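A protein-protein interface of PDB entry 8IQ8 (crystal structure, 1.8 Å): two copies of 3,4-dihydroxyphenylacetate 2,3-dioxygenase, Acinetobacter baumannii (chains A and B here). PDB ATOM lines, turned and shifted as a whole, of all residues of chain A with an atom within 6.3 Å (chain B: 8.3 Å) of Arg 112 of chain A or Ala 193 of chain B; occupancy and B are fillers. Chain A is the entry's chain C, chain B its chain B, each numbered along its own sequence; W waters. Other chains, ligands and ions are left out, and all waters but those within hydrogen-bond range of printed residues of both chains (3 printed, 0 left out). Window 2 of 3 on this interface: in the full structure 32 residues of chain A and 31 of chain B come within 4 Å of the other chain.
The side-chain carboxylate (OD1) of Asp 190 of chain B lies within hydrogen-bond range of the backbone NH (N) of Ala 63 of chain A, 2.9 Å away.
The side-chain carboxylate (OD1) of Asp 190 of chain B lies within salt-bridge range of the guanidinium group (NH1) of Arg 112 of chain A, at 2.8 Å.
Hydrophobic or aromatic side chains of chain A that line the printed part of chain B: Phe 64.
Along chain A the printed residues that touch a printed residue of chain B span positions 61 to 112.
Of the 14 printed residues of chain B, 3 touch a printed residue of chain A.
Among the printed residues, 5 pairs touch across the chains.
Among the printed residues, Asp or Glu carboxylates within 4 Å of a Lys or Arg side-chain nitrogen of the other chain: Arg 112 of chain A with Asp 190 of chain B (2.8 Å).
The side-chain hydroxyl (OG) of Ser 62 of chain A sits at hydrogen-bond distance from the guanidinium group (NH1) of Arg 112 of chain A (3.1 Å).
The backbone carbonyl oxygen of Arg 112 of chain A sits at hydrogen-bond distance from the backbone NH of Phe 64 of chain A, at 3.0 Å.
The backbone carbonyl oxygen (O) of Phe 64 of chain A lies within hydrogen-bond range of the backbone NH (N) of Gln 114 of chain A, 3.0 Å away.
Water W3 lies within hydrogen-bond range of O of Asn 61 of chain A (2.6 Å), O of Ile 188 of chain B (2.7 Å) and N of Asp 190 of chain B (3.3 Å).
Water W2 bridges the side-chain carboxylate of Asp 190 of chain B (2.6 Å) and the side-chain carboxylate of Asp 156 of chain A (2.9 Å).
Water W1 lies within hydrogen-bond range of OD2 of Asp 190 of chain B (2.7 Å), N of Arg 112 of chain A (2.9 Å) and OD2 of Asp 156 of chain A (3.3 Å).
Asn 61 of chain A touches Phe 187 of chain B (CB to CZ, 3.4 Å).
OD2 of Asp 190 of chain B touches CE2 of Phe 64 of chain A, at 3.8 Å.
Arg 112 of chain A touches Ala 193 of chain B (CZ to CB, 3.4 Å).
Printed residues of chain B within 4 Å of Asn 61 of chain A: Phe 187 (3.4 Å).
Printed residues of chain B within 4 Å of Ala 63 of chain A: Asp 190 (2.9 Å).
Of the printed residues of chain B, Phe 64 of chain A touches Asp 190.
Of the printed residues of chain B, Arg 112 of chain A touches Asp 190 (2.8 Å) and Ala 193 (3.4 Å).
Of chain A, only Arg 112 (3.4 Å) comes within 4 Å of Ala 193 of chain B.
The nearest printed residue of chain B that does not touch Phe 64 of chain A is Trp 191 of chain B (8.1 Å).
No position is printed for both chains.
Of the 5 pairs that touch across the chains among the printed residues, none has its exchanged pair printed and touching as well.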
ATOM      1  N   ASN A  61     -26.878 -26.729  10.476  1.00  0.00           N
ATOM      2  CA  ASN A  61     -25.481 -27.131  10.733  1.00  0.00           C
ATOM      3  C   ASN A  61     -24.535 -25.935  10.608  1.00  0.00           C
ATOM      4  O   ASN A  61     -23.457 -25.987  11.240  1.00  0.00           O
ATOM      5  CB  ASN A  61     -25.072 -28.240   9.786  1.00  0.00           C
ATOM      6  CG  ASN A  61     -25.823 -29.518  10.074  1.00  0.00           C
ATOM      7  OD1 ASN A  61     -25.835 -29.999  11.207  1.00  0.00           O
ATOM      8  ND2 ASN A  61     -26.443 -30.068   9.051  1.00  0.00           N
ATOM      9  N   SER A  62     -24.898 -24.941   9.792  1.00  0.00           N
ATOM     10  CA  SER A  62     -24.023 -23.814   9.365  1.00  0.00           C
ATOM     11  C   SER A  62     -24.803 -22.498   9.417  1.00  0.00           C
ATOM     12  O   SER A  62     -25.939 -22.457   8.862  1.00  0.00           O
ATOM     13  CB  SER A  62     -23.477 -24.081   7.988  1.00  0.00           C
ATOM     14  OG  SER A  62     -22.449 -23.157   7.690  1.00  0.00           O
ATOM     15  N   ALA A  63     -24.240 -21.498  10.104  1.00  0.00           N
ATOM     16  CA  ALA A  63     -24.790 -20.134  10.277  1.00  0.00           C
ATOM     17  C   ALA A  63     -26.123 -20.174  11.025  1.00  0.00           C
ATOM     18  O   ALA A  63     -26.645 -21.292  11.320  1.00  0.00           O
ATOM     19  CB  ALA A  63     -24.961 -19.462   8.930  1.00  0.00           C
ATOM     20  N   PHE A  64     -26.605 -18.983  11.382  1.00  0.00           N
ATOM     21  CA  PHE A  64     -27.942 -18.733  11.952  1.00  0.00           C
ATOM     22  C   PHE A  64     -28.845 -18.255  10.820  1.00  0.00           C
ATOM     23  O   PHE A  64     -28.474 -17.330  10.083  1.00  0.00           O
ATOM     24  CB  PHE A  64     -27.865 -17.725  13.087  1.00  0.00           C
ATOM     25  CG  PHE A  64     -26.981 -18.163  14.222  1.00  0.00           C
ATOM     26  CD1 PHE A  64     -27.514 -18.813  15.325  1.00  0.00           C
ATOM     27  CD2 PHE A  64     -25.612 -17.994  14.156  1.00  0.00           C
ATOM     28  CE1 PHE A  64     -26.705 -19.238  16.364  1.00  0.00           C
ATOM     29  CE2 PHE A  64     -24.795 -18.421  15.199  1.00  0.00           C
ATOM     30  CZ  PHE A  64     -25.342 -19.043  16.293  1.00  0.00           C
ATOM     31  N   HIS A  65     -30.020 -18.849  10.709  1.00  0.00           N
ATOM     32  CA  HIS A  65     -30.961 -18.522   9.616  1.00  0.00           C
ATOM     33  C   HIS A  65     -32.205 -17.841  10.158  1.00  0.00           C
ATOM     34  O   HIS A  65     -32.739 -18.291  11.195  1.00  0.00           O
ATOM     35  CB  HIS A  65     -31.246 -19.780   8.840  1.00  0.00           C
ATOM     36  CG  HIS A  65     -30.011 -20.355   8.244  1.00  0.00           C
ATOM     37  ND1 HIS A  65     -29.799 -20.368   6.871  1.00  0.00           N
ATOM     38  CD2 HIS A  65     -28.915 -20.911   8.808  1.00  0.00           C
ATOM     39  CE1 HIS A  65     -28.636 -20.952   6.617  1.00  0.00           C
ATOM     40  NE2 HIS A  65     -28.070 -21.281   7.790  1.00  0.00           N
ATOM     41  N   ILE A 106     -27.074  -8.142  13.233  1.00  0.00           N
ATOM     42  CA  ILE A 106     -26.434  -9.356  13.828  1.00  0.00           C
ATOM     43  C   ILE A 106     -25.129  -9.622  13.081  1.00  0.00           C
ATOM     44  O   ILE A 106     -24.176 -10.038  13.720  1.00  0.00           O
ATOM     45  CB  ILE A 106     -27.400 -10.553  13.832  1.00  0.00           C
ATOM     46  CG1 ILE A 106     -28.603 -10.246  14.735  1.00  0.00           C
ATOM     47  CG2 ILE A 106     -26.661 -11.822  14.251  1.00  0.00           C
ATOM     48  CD1 ILE A 106     -29.780 -11.179  14.570  1.00  0.00           C
ATOM     49  N   ALA A 107     -25.088  -9.369  11.775  1.00  0.00           N
ATOM     50  CA  ALA A 107     -23.872  -9.580  10.957  1.00  0.00           C
ATOM     51  C   ALA A 107     -22.778  -8.598  11.396  1.00  0.00           C
ATOM     52  O   ALA A 107     -21.617  -8.927  11.230  1.00  0.00           O
ATOM     53  CB  ALA A 107     -24.177  -9.447   9.483  1.00  0.00           C
ATOM     54  N   GLY A 110     -20.224 -10.040  14.024  1.00  0.00           N
ATOM     55  CA  GLY A 110     -19.309 -11.130  13.617  1.00  0.00           C
ATOM     56  C   GLY A 110     -20.030 -12.463  13.410  1.00  0.00           C
ATOM     57  O   GLY A 110     -19.475 -13.357  12.709  1.00  0.00           O
ATOM     58  N   VAL A 111     -21.240 -12.602  13.948  1.00  0.00           N
ATOM     59  CA  VAL A 111     -22.104 -13.810  13.757  1.00  0.00           C
ATOM     60  C   VAL A 111     -22.411 -14.017  12.267  1.00  0.00           C
ATOM     61  O   VAL A 111     -22.728 -13.029  11.578  1.00  0.00           O
ATOM     62  CB  VAL A 111     -23.393 -13.693  14.589  1.00  0.00           C
ATOM     63  CG1 VAL A 111     -24.417 -14.758  14.226  1.00  0.00           C
ATOM     64  CG2 VAL A 111     -23.074 -13.774  16.070  1.00  0.00           C
ATOM     65  N   ARG A 112     -22.318 -15.265  11.799  1.00  0.00           N
ATOM     66  CA  ARG A 112     -22.706 -15.659  10.424  1.00  0.00           C
ATOM     67  C   ARG A 112     -24.221 -15.802  10.404  1.00  0.00           C
ATOM     68  O   ARG A 112     -24.749 -16.648  11.151  1.00  0.00           O
ATOM     69  CB  ARG A 112     -22.035 -16.976  10.022  1.00  0.00           C
ATOM     70  CG  ARG A 112     -20.512 -16.917  10.002  1.00  0.00           C
ATOM     71  CD  ARG A 112     -19.894 -18.273   9.736  1.00  0.00           C
ATOM     72  NE  ARG A 112     -20.374 -18.741   8.436  1.00  0.00           N
ATOM     73  CZ  ARG A 112     -20.713 -19.995   8.114  1.00  0.00           C
ATOM     74  NH1 ARG A 112     -20.619 -20.982   8.996  1.00  0.00           N
ATOM     75  NH2 ARG A 112     -21.140 -20.245   6.887  1.00  0.00           N
ATOM     76  N   VAL A 113     -24.905 -15.000   9.599  1.00  0.00           N
ATOM     77  CA  VAL A 113     -26.383 -14.925   9.667  1.00  0.00           C
ATOM     78  C   VAL A 113     -26.913 -14.684   8.259  1.00  0.00           C
ATOM     79  O   VAL A 113     -26.299 -13.886   7.508  1.00  0.00           O
ATOM     80  CB  VAL A 113     -26.846 -13.860  10.670  1.00  0.00           C
ATOM     81  CG1 VAL A 113     -26.196 -12.503  10.427  1.00  0.00           C
ATOM     82  CG2 VAL A 113     -28.363 -13.771  10.689  1.00  0.00           C
ATOM     83  N   GLN A 114     -27.976 -15.402   7.905  1.00  0.00           N
ATOM     84  CA  GLN A 114     -28.653 -15.278   6.600  1.00  0.00           C
ATOM     85  C   GLN A 114     -30.140 -15.028   6.851  1.00  0.00           C
ATOM     86  O   GLN A 114     -30.725 -15.731   7.715  1.00  0.00           O
ATOM     87  CB  GLN A 114     -28.455 -16.538   5.754  1.00  0.00           C
ATOM     88  CG  GLN A 114     -27.006 -16.888   5.459  1.00  0.00           C
ATOM     89  CD  GLN A 114     -26.887 -18.247   4.796  1.00  0.00           C
ATOM     90  OE1 GLN A 114     -27.737 -18.657   4.000  1.00  0.00           O
ATOM     91  NE2 GLN A 114     -25.813 -18.964   5.096  1.00  0.00           N
ATOM     92  N   ASP A 156     -22.201 -17.119  20.355  1.00  0.00           N
ATOM     93  CA  ASP A 156     -22.731 -16.593  19.070  1.00  0.00           C
ATOM     94  C   ASP A 156     -24.253 -16.415  19.154  1.00  0.00           C
ATOM     95  O   ASP A 156     -24.764 -15.386  18.598  1.00  0.00           O
ATOM     96  CB  ASP A 156     -22.221 -17.399  17.873  1.00  0.00           C
ATOM     97  CG  ASP A 156     -20.814 -17.002  17.438  1.00  0.00           C
ATOM     98  OD1 ASP A 156     -20.314 -15.960  17.888  1.00  0.00           O
ATOM     99  OD2 ASP A 156     -20.209 -17.756  16.647  1.00  0.00           O
ATOM    100  N   PHE A 160     -26.301 -12.988  18.627  1.00  0.00           N
ATOM    101  CA  PHE A 160     -27.542 -12.951  17.809  1.00  0.00           C
ATOM    102  C   PHE A 160     -28.620 -12.160  18.577  1.00  0.00           C
ATOM    103  O   PHE A 160     -29.233 -11.262  17.980  1.00  0.00           O
ATOM    104  CB  PHE A 160     -28.028 -14.361  17.460  1.00  0.00           C
ATOM    105  CG  PHE A 160     -29.142 -14.392  16.451  1.00  0.00           C
ATOM    106  CD1 PHE A 160     -28.883 -14.731  15.133  1.00  0.00           C
ATOM    107  CD2 PHE A 160     -30.430 -14.028  16.801  1.00  0.00           C
ATOM    108  CE1 PHE A 160     -29.897 -14.741  14.183  1.00  0.00           C
ATOM    109  CE2 PHE A 160     -31.439 -14.027  15.853  1.00  0.00           C
ATOM    110  CZ  PHE A 160     -31.173 -14.381  14.550  1.00  0.00           C
ATOM    111  N   LEU B  81     -29.924 -25.323   3.824  1.00  0.00           N
ATOM    112  CA  LEU B  81     -29.289 -24.429   2.808  1.00  0.00           C
ATOM    113  C   LEU B  81     -30.343 -23.882   1.856  1.00  0.00           C
ATOM    114  O   LEU B  81     -30.292 -24.110   0.653  1.00  0.00           O
ATOM    115  CB  LEU B  81     -28.236 -25.203   2.015  1.00  0.00           C
ATOM    116  CG  LEU B  81     -27.013 -25.651   2.795  1.00  0.00           C
ATOM    117  CD1 LEU B  81     -26.151 -26.535   1.924  1.00  0.00           C
ATOM    118  CD2 LEU B  81     -26.208 -24.463   3.293  1.00  0.00           C
ATOM    119  N   PHE B 187     -20.091 -32.517  12.373  1.00  0.00           N
ATOM    120  CA  PHE B 187     -20.193 -31.440  11.357  1.00  0.00           C
ATOM    121  C   PHE B 187     -19.208 -30.308  11.716  1.00  0.00           C
ATOM    122  O   PHE B 187     -19.037 -30.034  12.899  1.00  0.00           O
ATOM    123  CB  PHE B 187     -21.638 -30.958  11.257  1.00  0.00           C
ATOM    124  CG  PHE B 187     -21.913 -30.165  10.012  1.00  0.00           C
ATOM    125  CD1 PHE B 187     -22.505 -30.772   8.917  1.00  0.00           C
ATOM    126  CD2 PHE B 187     -21.574 -28.830   9.935  1.00  0.00           C
ATOM    127  CE1 PHE B 187     -22.764 -30.043   7.760  1.00  0.00           C
ATOM    128  CE2 PHE B 187     -21.820 -28.099   8.774  1.00  0.00           C
ATOM    129  CZ  PHE B 187     -22.428 -28.709   7.696  1.00  0.00           C
ATOM    130  N   ILE B 188     -18.550 -29.697  10.723  1.00  0.00           N
ATOM    131  CA  ILE B 188     -17.526 -28.629  10.920  1.00  0.00           C
ATOM    132  C   ILE B 188     -18.138 -27.505  11.776  1.00  0.00           C
ATOM    133  O   ILE B 188     -19.305 -27.168  11.583  1.00  0.00           O
ATOM    134  CB  ILE B 188     -16.939 -28.181   9.558  1.00  0.00           C
ATOM    135  CG1 ILE B 188     -15.666 -27.341   9.693  1.00  0.00           C
ATOM    136  CG2 ILE B 188     -17.955 -27.453   8.690  1.00  0.00           C
ATOM    137  CD1 ILE B 188     -14.393 -28.122   9.798  1.00  0.00           C
ATOM    138  N   TRP B 189     -17.386 -26.991  12.743  1.00  0.00           N
ATOM    139  CA  TRP B 189     -17.812 -25.892  13.645  1.00  0.00           C
ATOM    140  C   TRP B 189     -18.136 -24.648  12.816  1.00  0.00           C
ATOM    141  O   TRP B 189     -17.449 -24.384  11.830  1.00  0.00           O
ATOM    142  CB  TRP B 189     -16.748 -25.571  14.684  1.00  0.00           C
ATOM    143  CG  TRP B 189     -16.315 -26.753  15.483  1.00  0.00           C
ATOM    144  CD1 TRP B 189     -15.070 -27.318  15.505  1.00  0.00           C
ATOM    145  CD2 TRP B 189     -17.130 -27.528  16.366  1.00  0.00           C
ATOM    146  NE1 TRP B 189     -15.055 -28.373  16.362  1.00  0.00           N
ATOM    147  CE2 TRP B 189     -16.299 -28.523  16.912  1.00  0.00           C
ATOM    148  CE3 TRP B 189     -18.459 -27.444  16.792  1.00  0.00           C
ATOM    149  CZ2 TRP B 189     -16.777 -29.456  17.825  1.00  0.00           C
ATOM    150  CZ3 TRP B 189     -18.926 -28.366  17.701  1.00  0.00           C
ATOM    151  CH2 TRP B 189     -18.094 -29.359  18.210  1.00  0.00           C
ATOM    152  N   ASP B 190     -19.169 -23.923  13.226  1.00  0.00           N
ATOM    153  CA  ASP B 190     -19.672 -22.710  12.537  1.00  0.00           C
ATOM    154  C   ASP B 190     -18.540 -21.678  12.371  1.00  0.00           C
ATOM    155  O   ASP B 190     -18.517 -21.009  11.333  1.00  0.00           O
ATOM    156  CB  ASP B 190     -20.861 -22.182  13.325  1.00  0.00           C
ATOM    157  CG  ASP B 190     -21.508 -20.954  12.733  1.00  0.00           C
ATOM    158  OD1 ASP B 190     -21.756 -20.948  11.523  1.00  0.00           O
ATOM    159  OD2 ASP B 190     -21.796 -20.049  13.512  1.00  0.00           O
ATOM    160  N   TRP B 191     -17.608 -21.582  13.323  1.00  0.00           N
ATOM    161  CA  TRP B 191     -16.490 -20.592  13.284  1.00  0.00           C
ATOM    162  C   TRP B 191     -15.355 -21.044  12.346  1.00  0.00           C
ATOM    163  O   TRP B 191     -14.382 -20.296  12.218  1.00  0.00           O
ATOM    164  CB  TRP B 191     -15.966 -20.305  14.698  1.00  0.00           C
ATOM    165  CG  TRP B 191     -15.585 -21.515  15.511  1.00  0.00           C
ATOM    166  CD1 TRP B 191     -14.344 -22.080  15.610  1.00  0.00           C
ATOM    167  CD2 TRP B 191     -16.433 -22.273  16.398  1.00  0.00           C
ATOM    168  NE1 TRP B 191     -14.368 -23.148  16.464  1.00  0.00           N
ATOM    169  CE2 TRP B 191     -15.634 -23.282  16.975  1.00  0.00           C
ATOM    170  CE3 TRP B 191     -17.794 -22.219  16.741  1.00  0.00           C
ATOM    171  CZ2 TRP B 191     -16.150 -24.212  17.873  1.00  0.00           C
ATOM    172  CZ3 TRP B 191     -18.302 -23.142  17.631  1.00  0.00           C
ATOM    173  CH2 TRP B 191     -17.485 -24.120  18.193  1.00  0.00           C
ATOM    174  N   GLU B 192     -15.459 -22.209  11.697  1.00  0.00           N
ATOM    175  CA  GLU B 192     -14.372 -22.771  10.843  1.00  0.00           C
ATOM    176  C   GLU B 192     -14.858 -22.853   9.396  1.00  0.00           C
ATOM    177  O   GLU B 192     -14.337 -23.689   8.641  1.00  0.00           O
ATOM    178  CB  GLU B 192     -13.929 -24.139  11.365  1.00  0.00           C
ATOM    179  CG  GLU B 192     -13.178 -24.065  12.680  1.00  0.00           C
ATOM    180  CD  GLU B 192     -12.688 -25.398  13.217  1.00  0.00           C
ATOM    181  OE1 GLU B 192     -12.854 -26.419  12.518  1.00  0.00           O
ATOM    182  OE2 GLU B 192     -12.138 -25.412  14.337  1.00  0.00           O
ATOM    183  N   ALA B 193     -15.797 -21.986   9.022  1.00  0.00           N
ATOM    184  CA  ALA B 193     -16.419 -21.922   7.680  1.00  0.00           C
ATOM    185  C   ALA B 193     -15.339 -21.761   6.603  1.00  0.00           C
ATOM    186  O   ALA B 193     -15.535 -22.281   5.478  1.00  0.00           O
ATOM    187  CB  ALA B 193     -17.411 -20.784   7.642  1.00  0.00           C
ATOM    188  N   GLN B 194     -14.249 -21.076   6.948  1.00  0.00           N
ATOM    189  CA  GLN B 194     -13.151 -20.675   6.027  1.00  0.00           C
ATOM    190  C   GLN B 194     -12.491 -21.911   5.409  1.00  0.00           C
ATOM    191  O   GLN B 194     -12.091 -21.827   4.230  1.00  0.00           O
ATOM    192  CB  GLN B 194     -12.128 -19.818   6.775  1.00  0.00           C
ATOM    193  CG  GLN B 194     -12.681 -18.473   7.239  1.00  0.00           C
ATOM    194  CD  GLN B 194     -13.167 -17.599   6.104  1.00  0.00           C
ATOM    195  OE1 GLN B 194     -14.220 -17.841   5.512  1.00  0.00           O
ATOM    196  NE2 GLN B 194     -12.408 -16.556   5.800  1.00  0.00           N
ATOM    197  N   ARG B 195     -12.422 -23.023   6.148  1.00  0.00           N
ATOM    198  CA  ARG B 195     -11.716 -24.262   5.715  1.00  0.00           C
ATOM    199  C   ARG B 195     -12.510 -24.980   4.605  1.00  0.00           C
ATOM    200  O   ARG B 195     -11.932 -25.859   3.940  1.00  0.00           O
ATOM    201  CB  ARG B 195     -11.448 -25.159   6.927  1.00  0.00           C
ATOM    202  CG  ARG B 195     -10.943 -24.401   8.149  1.00  0.00           C
ATOM    203  CD  ARG B 195     -10.217 -25.224   9.197  1.00  0.00           C
ATOM    204  NE  ARG B 195     -10.420 -26.659   9.036  1.00  0.00           N
ATOM    205  CZ  ARG B 195     -10.570 -27.536  10.028  1.00  0.00           C
ATOM    206  NH1 ARG B 195     -10.562 -27.130  11.287  1.00  0.00           N
ATOM    207  NH2 ARG B 195     -10.750 -28.821   9.751  1.00  0.00           N
ATOM    208  N   GLY B 196     -13.772 -24.605   4.379  1.00  0.00           N
ATOM    209  CA  GLY B 196     -14.582 -25.116   3.252  1.00  0.00           C
ATOM    210  C   GLY B 196     -15.118 -26.522   3.507  1.00  0.00           C
ATOM    211  O   GLY B 196     -15.196 -26.950   4.676  1.00  0.00           O
ATOM    212  N   MET B 197     -15.397 -27.245   2.427  1.00  0.00           N
ATOM    213  CA  MET B 197     -16.363 -28.364   2.396  1.00  0.00           C
ATOM    214  C   MET B 197     -15.653 -29.726   2.339  1.00  0.00           C
ATOM    215  O   MET B 197     -16.369 -30.739   2.411  1.00  0.00           O
ATOM    216  CB  MET B 197     -17.266 -28.201   1.166  1.00  0.00           C
ATOM    217  CG  MET B 197     -18.720 -28.345   1.473  1.00  0.00           C
ATOM    218  SD  MET B 197     -19.796 -27.601   0.212  1.00  0.00           S
ATOM    219  CE  MET B 197     -20.372 -26.153   1.103  1.00  0.00           C
ATOM    220  N   ASP B 198     -14.318 -29.762   2.230  1.00  0.00           N
ATOM    221  CA  ASP B 198     -13.571 -31.001   1.903  1.00  0.00           C
ATOM    222  C   ASP B 198     -12.590 -31.373   3.017  1.00  0.00           C
ATOM    223  O   ASP B 198     -11.561 -31.950   2.697  1.00  0.00           O
ATOM    224  CB  ASP B 198     -12.878 -30.856   0.551  1.00  0.00           C
ATOM    225  CG  ASP B 198     -13.886 -30.635  -0.549  1.00  0.00           C
ATOM    226  OD1 ASP B 198     -14.900 -31.333  -0.548  1.00  0.00           O
ATOM    227  OD2 ASP B 198     -13.677 -29.729  -1.329  1.00  0.00           O
ATOM    228  N   THR B 199     -12.937 -31.118   4.278  1.00  0.00           N
ATOM    229  CA  THR B 199     -12.079 -31.449   5.437  1.00  0.00           C
ATOM    230  C   THR B 199     -12.901 -32.152   6.510  1.00  0.00           C
ATOM    231  O   THR B 199     -14.119 -31.902   6.579  1.00  0.00           O
ATOM    232  CB  THR B 199     -11.422 -30.192   6.026  1.00  0.00           C
ATOM    233  OG1 THR B 199     -12.408 -29.443   6.745  1.00  0.00           O
ATOM    234  CG2 THR B 199     -10.803 -29.311   4.966  1.00  0.00           C
HETATM  235  O   HOH W   1     -21.677 -17.400  13.694  1.00  0.00           O
HETATM  236  O   HOH W   2     -21.333 -20.379  16.097  1.00  0.00           O
HETATM  237  O   HOH W   3     -20.971 -25.232  10.748  1.00  0.00           O
